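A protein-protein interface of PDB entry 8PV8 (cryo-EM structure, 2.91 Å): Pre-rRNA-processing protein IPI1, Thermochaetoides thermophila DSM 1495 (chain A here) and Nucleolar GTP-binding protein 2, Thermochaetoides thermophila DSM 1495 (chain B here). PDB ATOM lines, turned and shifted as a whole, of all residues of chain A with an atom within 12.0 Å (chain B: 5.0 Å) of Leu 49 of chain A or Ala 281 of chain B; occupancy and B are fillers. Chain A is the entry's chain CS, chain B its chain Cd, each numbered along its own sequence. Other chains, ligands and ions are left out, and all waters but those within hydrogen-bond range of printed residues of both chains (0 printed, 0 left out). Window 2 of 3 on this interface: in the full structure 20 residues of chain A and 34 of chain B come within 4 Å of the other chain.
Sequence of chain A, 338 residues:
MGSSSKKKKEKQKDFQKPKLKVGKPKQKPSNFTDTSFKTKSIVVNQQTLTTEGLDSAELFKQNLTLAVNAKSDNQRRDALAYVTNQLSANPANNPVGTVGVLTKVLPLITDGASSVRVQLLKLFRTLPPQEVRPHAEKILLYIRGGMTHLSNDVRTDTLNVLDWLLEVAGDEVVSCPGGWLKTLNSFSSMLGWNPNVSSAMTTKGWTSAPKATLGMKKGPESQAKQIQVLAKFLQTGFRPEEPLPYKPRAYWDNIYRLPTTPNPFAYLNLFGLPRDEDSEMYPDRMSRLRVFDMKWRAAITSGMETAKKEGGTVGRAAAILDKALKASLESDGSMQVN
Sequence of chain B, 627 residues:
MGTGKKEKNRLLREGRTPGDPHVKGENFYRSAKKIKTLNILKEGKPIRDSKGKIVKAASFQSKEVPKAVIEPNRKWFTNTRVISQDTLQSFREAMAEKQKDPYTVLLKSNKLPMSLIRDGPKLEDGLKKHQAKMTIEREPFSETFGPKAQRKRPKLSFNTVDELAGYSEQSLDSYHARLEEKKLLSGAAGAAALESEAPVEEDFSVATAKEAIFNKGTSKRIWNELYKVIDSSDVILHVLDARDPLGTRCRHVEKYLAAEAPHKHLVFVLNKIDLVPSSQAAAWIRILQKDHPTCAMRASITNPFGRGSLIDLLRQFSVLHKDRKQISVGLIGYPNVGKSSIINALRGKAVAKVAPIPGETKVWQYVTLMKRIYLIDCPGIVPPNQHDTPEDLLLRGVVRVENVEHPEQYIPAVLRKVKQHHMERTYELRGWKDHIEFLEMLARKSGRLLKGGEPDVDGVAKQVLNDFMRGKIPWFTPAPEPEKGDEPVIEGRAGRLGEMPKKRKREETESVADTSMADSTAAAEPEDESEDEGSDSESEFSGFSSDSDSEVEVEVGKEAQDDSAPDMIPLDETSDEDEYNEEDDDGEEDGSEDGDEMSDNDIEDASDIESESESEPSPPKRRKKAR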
ATOM      1  N   VAL A  44     -11.426  30.356  11.393  1.00  0.00           N
ATOM      2  CA  VAL A  44     -12.529  29.766  10.645  1.00  0.00           C
ATOM      3  C   VAL A  44     -12.864  28.429  11.289  1.00  0.00           C
ATOM      4  O   VAL A  44     -12.037  27.510  11.297  1.00  0.00           O
ATOM      5  CB  VAL A  44     -12.177  29.593   9.160  1.00  0.00           C
ATOM      6  CG1 VAL A  44     -13.354  29.001   8.404  1.00  0.00           C
ATOM      7  CG2 VAL A  44     -11.761  30.922   8.554  1.00  0.00           C
ATOM      8  N   ASN A  45     -14.076  28.319  11.822  1.00  0.00           N
ATOM      9  CA  ASN A  45     -14.504  27.144  12.578  1.00  0.00           C
ATOM     10  C   ASN A  45     -15.209  26.187  11.626  1.00  0.00           C
ATOM     11  O   ASN A  45     -16.437  26.134  11.562  1.00  0.00           O
ATOM     12  CB  ASN A  45     -15.406  27.556  13.733  1.00  0.00           C
ATOM     13  CG  ASN A  45     -14.768  28.597  14.620  1.00  0.00           C
ATOM     14  OD1 ASN A  45     -13.601  28.951  14.445  1.00  0.00           O
ATOM     15  ND2 ASN A  45     -15.536  29.116  15.566  1.00  0.00           N
ATOM     16  N   GLN A  46     -14.417  25.424  10.877  1.00  0.00           N
ATOM     17  CA  GLN A  46     -14.959  24.398   9.998  1.00  0.00           C
ATOM     18  C   GLN A  46     -14.031  23.196  10.026  1.00  0.00           C
ATOM     19  O   GLN A  46     -12.806  23.354   9.988  1.00  0.00           O
ATOM     20  CB  GLN A  46     -15.125  24.916   8.567  1.00  0.00           C
ATOM     21  CG  GLN A  46     -15.967  24.010   7.686  1.00  0.00           C
ATOM     22  CD  GLN A  46     -16.213  24.593   6.313  1.00  0.00           C
ATOM     23  OE1 GLN A  46     -15.477  25.466   5.856  1.00  0.00           O
ATOM     24  NE2 GLN A  46     -17.256  24.115   5.646  1.00  0.00           N
ATOM     25  N   GLN A  47     -14.613  22.005  10.096  1.00  0.00           N
ATOM     26  CA  GLN A  47     -13.827  20.785  10.153  1.00  0.00           C
ATOM     27  C   GLN A  47     -13.245  20.456   8.781  1.00  0.00           C
ATOM     28  O   GLN A  47     -13.625  21.032   7.759  1.00  0.00           O
ATOM     29  CB  GLN A  47     -14.682  19.621  10.651  1.00  0.00           C
ATOM     30  CG  GLN A  47     -15.405  19.898  11.958  1.00  0.00           C
ATOM     31  CD  GLN A  47     -16.401  18.812  12.313  1.00  0.00           C
ATOM     32  OE1 GLN A  47     -16.536  17.821  11.597  1.00  0.00           O
ATOM     33  NE2 GLN A  47     -17.106  18.995  13.424  1.00  0.00           N
ATOM     34  N   THR A  48     -12.299  19.521   8.776  1.00  0.00           N
ATOM     35  CA  THR A  48     -11.731  19.034   7.531  1.00  0.00           C
ATOM     36  C   THR A  48     -12.787  18.269   6.737  1.00  0.00           C
ATOM     37  O   THR A  48     -13.581  17.503   7.286  1.00  0.00           O
ATOM     38  CB  THR A  48     -10.521  18.141   7.808  1.00  0.00           C
ATOM     39  OG1 THR A  48      -9.717  18.734   8.835  1.00  0.00           O
ATOM     40  CG2 THR A  48      -9.676  17.975   6.555  1.00  0.00           C
ATOM     41  N   LEU A  49     -12.801  18.506   5.428  1.00  0.00           N
ATOM     42  CA  LEU A  49     -13.835  17.953   4.561  1.00  0.00           C
ATOM     43  C   LEU A  49     -13.675  16.457   4.322  1.00  0.00           C
ATOM     44  O   LEU A  49     -14.662  15.715   4.375  1.00  0.00           O
ATOM     45  CB  LEU A  49     -13.844  18.691   3.220  1.00  0.00           C
ATOM     46  CG  LEU A  49     -14.826  19.851   3.036  1.00  0.00           C
ATOM     47  CD1 LEU A  49     -14.629  20.940   4.078  1.00  0.00           C
ATOM     48  CD2 LEU A  49     -14.684  20.428   1.641  1.00  0.00           C
ATOM     49  N   THR A  50     -12.450  15.993   4.062  1.00  0.00           N
ATOM     50  CA  THR A  50     -12.264  14.610   3.635  1.00  0.00           C
ATOM     51  C   THR A  50     -12.370  13.630   4.802  1.00  0.00           C
ATOM     52  O   THR A  50     -12.867  12.511   4.623  1.00  0.00           O
ATOM     53  CB  THR A  50     -10.928  14.462   2.897  1.00  0.00           C
ATOM     54  OG1 THR A  50     -10.746  13.099   2.493  1.00  0.00           O
ATOM     55  CG2 THR A  50      -9.748  14.930   3.748  1.00  0.00           C
ATOM     56  N   THR A  51     -11.936  14.042   5.998  1.00  0.00           N
ATOM     57  CA  THR A  51     -11.923  13.222   7.219  1.00  0.00           C
ATOM     58  C   THR A  51     -11.218  11.883   7.002  1.00  0.00           C
ATOM     59  O   THR A  51     -11.673  10.828   7.451  1.00  0.00           O
ATOM     60  CB  THR A  51     -13.337  13.002   7.767  1.00  0.00           C
ATOM     61  OG1 THR A  51     -14.064  12.122   6.899  1.00  0.00           O
ATOM     62  CG2 THR A  51     -14.081  14.320   7.881  1.00  0.00           C
ATOM     63  N   GLU A  52     -10.087  11.927   6.295  1.00  0.00           N
ATOM     64  CA  GLU A  52      -9.309  10.724   6.038  1.00  0.00           C
ATOM     65  C   GLU A  52      -7.999  10.665   6.809  1.00  0.00           C
ATOM     66  O   GLU A  52      -7.465   9.568   6.999  1.00  0.00           O
ATOM     67  CB  GLU A  52      -9.010  10.581   4.537  1.00  0.00           C
ATOM     68  CG  GLU A  52      -8.065  11.629   3.972  1.00  0.00           C
ATOM     69  CD  GLU A  52      -7.992  11.591   2.458  1.00  0.00           C
ATOM     70  OE1 GLU A  52      -8.723  10.785   1.846  1.00  0.00           O
ATOM     71  OE2 GLU A  52      -7.203  12.369   1.880  1.00  0.00           O
ATOM     72  N   GLY A  53      -7.469  11.806   7.255  1.00  0.00           N
ATOM     73  CA  GLY A  53      -6.243  11.781   8.034  1.00  0.00           C
ATOM     74  C   GLY A  53      -6.470  11.323   9.462  1.00  0.00           C
ATOM     75  O   GLY A  53      -5.537  10.889  10.141  1.00  0.00           O
ATOM     76  N   LEU A  54      -7.710  11.420   9.937  1.00  0.00           N
ATOM     77  CA  LEU A  54      -8.029  11.001  11.294  1.00  0.00           C
ATOM     78  C   LEU A  54      -8.004   9.482  11.408  1.00  0.00           C
ATOM     79  O   LEU A  54      -8.337   8.764  10.461  1.00  0.00           O
ATOM     80  CB  LEU A  54      -9.399  11.542  11.704  1.00  0.00           C
ATOM     81  CG  LEU A  54      -9.475  13.043  11.984  1.00  0.00           C
ATOM     82  CD1 LEU A  54     -10.890  13.556  11.776  1.00  0.00           C
ATOM     83  CD2 LEU A  54      -8.988  13.352  13.391  1.00  0.00           C
ATOM     84  N   LEU A  59     -12.340   8.584  14.592  1.00  0.00           N
ATOM     85  CA  LEU A  59     -13.591   8.352  13.871  1.00  0.00           C
ATOM     86  C   LEU A  59     -14.656   7.765  14.789  1.00  0.00           C
ATOM     87  O   LEU A  59     -15.821   8.179  14.744  1.00  0.00           O
ATOM     88  CB  LEU A  59     -13.349   7.425  12.679  1.00  0.00           C
ATOM     89  CG  LEU A  59     -13.246   8.050  11.287  1.00  0.00           C
ATOM     90  CD1 LEU A  59     -12.163   9.112  11.239  1.00  0.00           C
ATOM     91  CD2 LEU A  59     -12.994   6.976  10.241  1.00  0.00           C
ATOM     92  N   GLN A  62     -15.772  10.593  17.262  1.00  0.00           N
ATOM     93  CA  GLN A  62     -16.552  11.609  16.565  1.00  0.00           C
ATOM     94  C   GLN A  62     -17.929  11.089  16.178  1.00  0.00           C
ATOM     95  O   GLN A  62     -18.929  11.800  16.320  1.00  0.00           O
ATOM     96  CB  GLN A  62     -15.799  12.093  15.325  1.00  0.00           C
ATOM     97  CG  GLN A  62     -14.710  13.112  15.614  1.00  0.00           C
ATOM     98  CD  GLN A  62     -14.402  13.985  14.414  1.00  0.00           C
ATOM     99  OE1 GLN A  62     -14.332  13.505  13.283  1.00  0.00           O
ATOM    100  NE2 GLN A  62     -14.215  15.278  14.656  1.00  0.00           N
ATOM    101  N   ASN A  63     -18.008   9.846  15.698  1.00  0.00           N
ATOM    102  CA  ASN A  63     -19.301   9.307  15.303  1.00  0.00           C
ATOM    103  C   ASN A  63     -20.177   9.020  16.514  1.00  0.00           C
ATOM    104  O   ASN A  63     -21.401   9.165  16.445  1.00  0.00           O
ATOM    105  CB  ASN A  63     -19.104   8.061  14.446  1.00  0.00           C
ATOM    106  CG  ASN A  63     -18.841   8.399  12.991  1.00  0.00           C
ATOM    107  OD1 ASN A  63     -19.766   8.694  12.235  1.00  0.00           O
ATOM    108  ND2 ASN A  63     -17.572   8.387  12.600  1.00  0.00           N
ATOM    109  N   LEU A  66     -21.532  12.520  17.399  1.00  0.00           N
ATOM    110  CA  LEU A  66     -22.610  12.900  16.488  1.00  0.00           C
ATOM    111  C   LEU A  66     -23.858  12.050  16.706  1.00  0.00           C
ATOM    112  O   LEU A  66     -24.980  12.539  16.543  1.00  0.00           O
ATOM    113  CB  LEU A  66     -22.144  12.824  15.032  1.00  0.00           C
ATOM    114  CG  LEU A  66     -21.514  14.080  14.411  1.00  0.00           C
ATOM    115  CD1 LEU A  66     -20.147  14.433  14.969  1.00  0.00           C
ATOM    116  CD2 LEU A  66     -21.442  13.922  12.899  1.00  0.00           C
ATOM    117  N   GLN A  75     -28.694  11.288  10.351  1.00  0.00           N
ATOM    118  CA  GLN A  75     -27.298  11.349  10.775  1.00  0.00           C
ATOM    119  C   GLN A  75     -27.060  10.504  12.022  1.00  0.00           C
ATOM    120  O   GLN A  75     -26.045   9.801  12.119  1.00  0.00           O
ATOM    121  CB  GLN A  75     -26.889  12.801  11.018  1.00  0.00           C
ATOM    122  CG  GLN A  75     -25.392  13.048  10.968  1.00  0.00           C
ATOM    123  CD  GLN A  75     -25.058  14.467  10.548  1.00  0.00           C
ATOM    124  OE1 GLN A  75     -25.948  15.258  10.239  1.00  0.00           O
ATOM    125  NE2 GLN A  75     -23.771  14.792  10.523  1.00  0.00           N
ATOM    126  N   LEU B 270     -15.163  28.921  -1.053  1.00  0.00           N
ATOM    127  CA  LEU B 270     -15.114  27.924  -2.113  1.00  0.00           C
ATOM    128  C   LEU B 270     -16.479  27.253  -2.201  1.00  0.00           C
ATOM    129  O   LEU B 270     -16.832  26.430  -1.347  1.00  0.00           O
ATOM    130  CB  LEU B 270     -14.013  26.905  -1.837  1.00  0.00           C
ATOM    131  CG  LEU B 270     -13.591  26.014  -3.003  1.00  0.00           C
ATOM    132  CD1 LEU B 270     -12.968  26.848  -4.103  1.00  0.00           C
ATOM    133  CD2 LEU B 270     -12.627  24.941  -2.532  1.00  0.00           C
ATOM    134  N   ILE B 273     -18.743  22.608  -3.824  1.00  0.00           N
ATOM    135  CA  ILE B 273     -17.857  21.504  -3.461  1.00  0.00           C
ATOM    136  C   ILE B 273     -18.504  20.145  -3.661  1.00  0.00           C
ATOM    137  O   ILE B 273     -17.818  19.122  -3.551  1.00  0.00           O
ATOM    138  CB  ILE B 273     -17.380  21.608  -2.000  1.00  0.00           C
ATOM    139  CG1 ILE B 273     -18.546  21.368  -1.047  1.00  0.00           C
ATOM    140  CG2 ILE B 273     -16.752  22.965  -1.742  1.00  0.00           C
ATOM    141  CD1 ILE B 273     -18.115  21.181   0.371  1.00  0.00           C
ATOM    142  N   VAL B 276     -17.034  18.377  -6.877  1.00  0.00           N
ATOM    143  CA  VAL B 276     -15.630  17.969  -6.869  1.00  0.00           C
ATOM    144  C   VAL B 276     -15.458  16.873  -5.824  1.00  0.00           C
ATOM    145  O   VAL B 276     -16.289  16.758  -4.911  1.00  0.00           O
ATOM    146  CB  VAL B 276     -14.697  19.161  -6.588  1.00  0.00           C
ATOM    147  CG1 VAL B 276     -14.780  20.190  -7.704  1.00  0.00           C
ATOM    148  CG2 VAL B 276     -15.021  19.790  -5.247  1.00  0.00           C
ATOM    149  N   PRO B 277     -14.431  16.026  -5.931  1.00  0.00           N
ATOM    150  CA  PRO B 277     -14.152  15.073  -4.850  1.00  0.00           C
ATOM    151  C   PRO B 277     -13.738  15.785  -3.571  1.00  0.00           C
ATOM    152  O   PRO B 277     -13.207  16.898  -3.600  1.00  0.00           O
ATOM    153  CB  PRO B 277     -13.012  14.220  -5.418  1.00  0.00           C
ATOM    154  CG  PRO B 277     -13.171  14.330  -6.892  1.00  0.00           C
ATOM    155  CD  PRO B 277     -13.623  15.737  -7.128  1.00  0.00           C
ATOM    156  N   SER B 278     -14.003  15.131  -2.436  1.00  0.00           N
ATOM    157  CA  SER B 278     -13.786  15.761  -1.136  1.00  0.00           C
ATOM    158  C   SER B 278     -12.307  15.983  -0.842  1.00  0.00           C
ATOM    159  O   SER B 278     -11.945  16.998  -0.236  1.00  0.00           O
ATOM    160  CB  SER B 278     -14.425  14.913  -0.037  1.00  0.00           C
ATOM    161  OG  SER B 278     -14.369  15.577   1.213  1.00  0.00           O
ATOM    162  N   SER B 279     -11.445  15.045  -1.247  1.00  0.00           N
ATOM    163  CA  SER B 279     -10.010  15.200  -1.020  1.00  0.00           C
ATOM    164  C   SER B 279      -9.446  16.364  -1.826  1.00  0.00           C
ATOM    165  O   SER B 279      -8.619  17.140  -1.327  1.00  0.00           O
ATOM    166  CB  SER B 279      -9.284  13.901  -1.371  1.00  0.00           C
ATOM    167  OG  SER B 279      -9.454  13.583  -2.741  1.00  0.00           O
ATOM    168  N   GLN B 280      -9.888  16.502  -3.079  1.00  0.00           N
ATOM    169  CA  GLN B 280      -9.473  17.637  -3.897  1.00  0.00           C
ATOM    170  C   GLN B 280      -9.970  18.950  -3.309  1.00  0.00           C
ATOM    171  O   GLN B 280      -9.244  19.951  -3.313  1.00  0.00           O
ATOM    172  CB  GLN B 280      -9.979  17.468  -5.330  1.00  0.00           C
ATOM    173  CG  GLN B 280      -9.551  16.174  -5.998  1.00  0.00           C
ATOM    174  CD  GLN B 280      -8.116  16.210  -6.489  1.00  0.00           C
ATOM    175  OE1 GLN B 280      -7.463  17.252  -6.465  1.00  0.00           O
ATOM    176  NE2 GLN B 280      -7.620  15.065  -6.941  1.00  0.00           N
ATOM    177  N   ALA B 281     -11.199  18.954  -2.787  1.00  0.00           N
ATOM    178  CA  ALA B 281     -11.737  20.152  -2.150  1.00  0.00           C
ATOM    179  C   ALA B 281     -10.927  20.533  -0.918  1.00  0.00           C
ATOM    180  O   ALA B 281     -10.632  21.712  -0.701  1.00  0.00           O
ATOM    181  CB  ALA B 281     -13.206  19.935  -1.786  1.00  0.00           C
ATOM    182  N   ALA B 282     -10.539  19.541  -0.109  1.00  0.00           N
ATOM    183  CA  ALA B 282      -9.726  19.818   1.073  1.00  0.00           C
ATOM    184  C   ALA B 282      -8.344  20.338   0.692  1.00  0.00           C
ATOM    185  O   ALA B 282      -7.804  21.236   1.353  1.00  0.00           O
ATOM    186  CB  ALA B 282      -9.608  18.561   1.934  1.00  0.00           C
ATOM    187  N   ALA B 283      -7.755  19.785  -0.374  1.00  0.00           N
ATOM    188  CA  ALA B 283      -6.467  20.283  -0.852  1.00  0.00           C
ATOM    189  C   ALA B 283      -6.574  21.725  -1.341  1.00  0.00           C
ATOM    190  O   ALA B 283      -5.682  22.544  -1.078  1.00  0.00           O
ATOM    191  CB  ALA B 283      -5.934  19.378  -1.960  1.00  0.00           C
ATOM    192  N   TRP B 284      -7.661  22.052  -2.047  1.00  0.00           N
ATOM    193  CA  TRP B 284      -7.865  23.427  -2.490  1.00  0.00           C
ATOM    194  C   TRP B 284      -8.076  24.369  -1.311  1.00  0.00           C
ATOM    195  O   TRP B 284      -7.596  25.508  -1.338  1.00  0.00           O
ATOM    196  CB  TRP B 284      -9.051  23.516  -3.450  1.00  0.00           C
ATOM    197  CG  TRP B 284      -8.762  23.048  -4.853  1.00  0.00           C
ATOM    198  CD1 TRP B 284      -9.375  22.023  -5.510  1.00  0.00           C
ATOM    199  CD2 TRP B 284      -7.779  23.570  -5.759  1.00  0.00           C
ATOM    200  NE1 TRP B 284      -8.849  21.880  -6.768  1.00  0.00           N
ATOM    201  CE2 TRP B 284      -7.867  22.817  -6.946  1.00  0.00           C
ATOM    202  CE3 TRP B 284      -6.843  24.604  -5.686  1.00  0.00           C
ATOM    203  CZ2 TRP B 284      -7.053  23.065  -8.046  1.00  0.00           C
ATOM    204  CZ3 TRP B 284      -6.034  24.840  -6.777  1.00  0.00           C
ATOM    205  CH2 TRP B 284      -6.145  24.078  -7.942  1.00  0.00           C
ATOM    206  N   ILE B 285      -8.789  23.912  -0.275  1.00  0.00           N
ATOM    207  CA  ILE B 285      -8.949  24.708   0.943  1.00  0.00           C
ATOM    208  C   ILE B 285      -7.600  24.959   1.605  1.00  0.00           C
ATOM    209  O   ILE B 285      -7.334  26.064   2.087  1.00  0.00           O
ATOM    210  CB  ILE B 285      -9.951  24.034   1.906  1.00  0.00           C
ATOM    211  CG1 ILE B 285     -11.359  24.031   1.302  1.00  0.00           C
ATOM    212  CG2 ILE B 285      -9.941  24.685   3.288  1.00  0.00           C
ATOM    213  CD1 ILE B 285     -12.146  25.306   1.527  1.00  0.00           C
ATOM    214  N   ALA B 296     -15.541  26.534   3.161  1.00  0.00           N
ATOM    215  CA  ALA B 296     -16.145  25.636   2.192  1.00  0.00           C
ATOM    216  C   ALA B 296     -17.656  25.812   2.232  1.00  0.00           C
ATOM    217  O   ALA B 296     -18.237  26.052   3.294  1.00  0.00           O
ATOM    218  CB  ALA B 296     -15.775  24.178   2.472  1.00  0.00           C
ATOM    219  N   PHE B 305     -24.233  23.627   3.241  1.00  0.00           N
ATOM    220  CA  PHE B 305     -23.063  23.168   3.975  1.00  0.00           C
ATOM    221  C   PHE B 305     -22.113  24.340   4.165  1.00  0.00           C
ATOM    222  O   PHE B 305     -21.914  25.131   3.241  1.00  0.00           O
ATOM    223  CB  PHE B 305     -22.361  22.020   3.246  1.00  0.00           C
ATOM    224  CG  PHE B 305     -21.100  21.563   3.915  1.00  0.00           C
ATOM    225  CD1 PHE B 305     -21.145  20.836   5.092  1.00  0.00           C
ATOM    226  CD2 PHE B 305     -19.867  21.858   3.364  1.00  0.00           C
ATOM    227  CE1 PHE B 305     -19.980  20.420   5.708  1.00  0.00           C
ATOM    228  CE2 PHE B 305     -18.701  21.441   3.971  1.00  0.00           C
ATOM    229  CZ  PHE B 305     -18.757  20.720   5.144  1.00  0.00           C
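OE1 of Gln 46 of chain A lies within hydrogen-bond range of N of Ala 296 of chain B (2.9 Å).
The side-chain hydroxyl (OG) of Ser 278 of chain B lies close to the backbone NH (N) of Thr 50 of chain A, at 3.5 Å.
The backbone carbonyl oxygen (O) of Leu 49 of chain A lies within hydrogen-bond range of the side-chain hydroxyl (OG) of Ser 278 of chain B.
The side-chain hydroxyl (OG1) of Thr 50 of chain A lies close to the side-chain carboxylate (OE1) of Glu 52 of chain A (3.1 Å).
Among the printed residues, merely in contact across the chains: Gln 46 of chain A with Phe 305 of chain B, Leu 49 of chain A with Ile 273 of chain B, Leu 49 of chain A with Ala 281 of chain B and Leu 49 of chain A with Ala 296 of chain B.
Leu 49 of chain A touches four residues of chain B.
Of chain A, only Leu 49 (3.8 Å) comes within 4 Å of Ala 281 of chain B.
No residue of chain A comes within 4 Å of Pro 277 of chain B.
Ser 278 of chain B touches just these residues of chain A: Leu 49 and Thr 50.
No residue of chain A comes within 4 Å of Gln 280 of chain B.
No residue of chain A comes within 4 Å of Ala 282 of chain B.
No residue of chain A comes within 4 Å of Ala 283 of chain B.
Of the printed residues of chain B, Thr 50 of chain A touches Ser 278 (3.4 Å).
Of the printed residues of chain A, Phe 305 of chain B touches Gln 46 (3.5 Å).
Thr 51 of chain A touches none of the printed residues of chain B.
The nearest residue of chain A that does not touch Ala 281 of chain B is Thr 50 of chain A (6.9 Å).
Of the 14 printed residues of chain B, 5 touch a printed residue of chain A.
Hydrophobic or aromatic side chains of chain B within 4 Å of the printed part of chain A: Ile 273, Ala 281, Ala 296 and Phe 305.
Of the 16 printed residues of chain A, 3 touch a printed residue of chain B.
Printed residues of chain A that touch a printed residue of chain B: Gln 46, Leu 49 and Thr 50.
Hydrophobic or aromatic side chains of chain A within 4 Å of the printed part of chain B: Leu 49.
Among the printed residues, no Asp or Glu carboxylate lies within 4 Å of a Lys or Arg side-chain nitrogen of the other chain.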
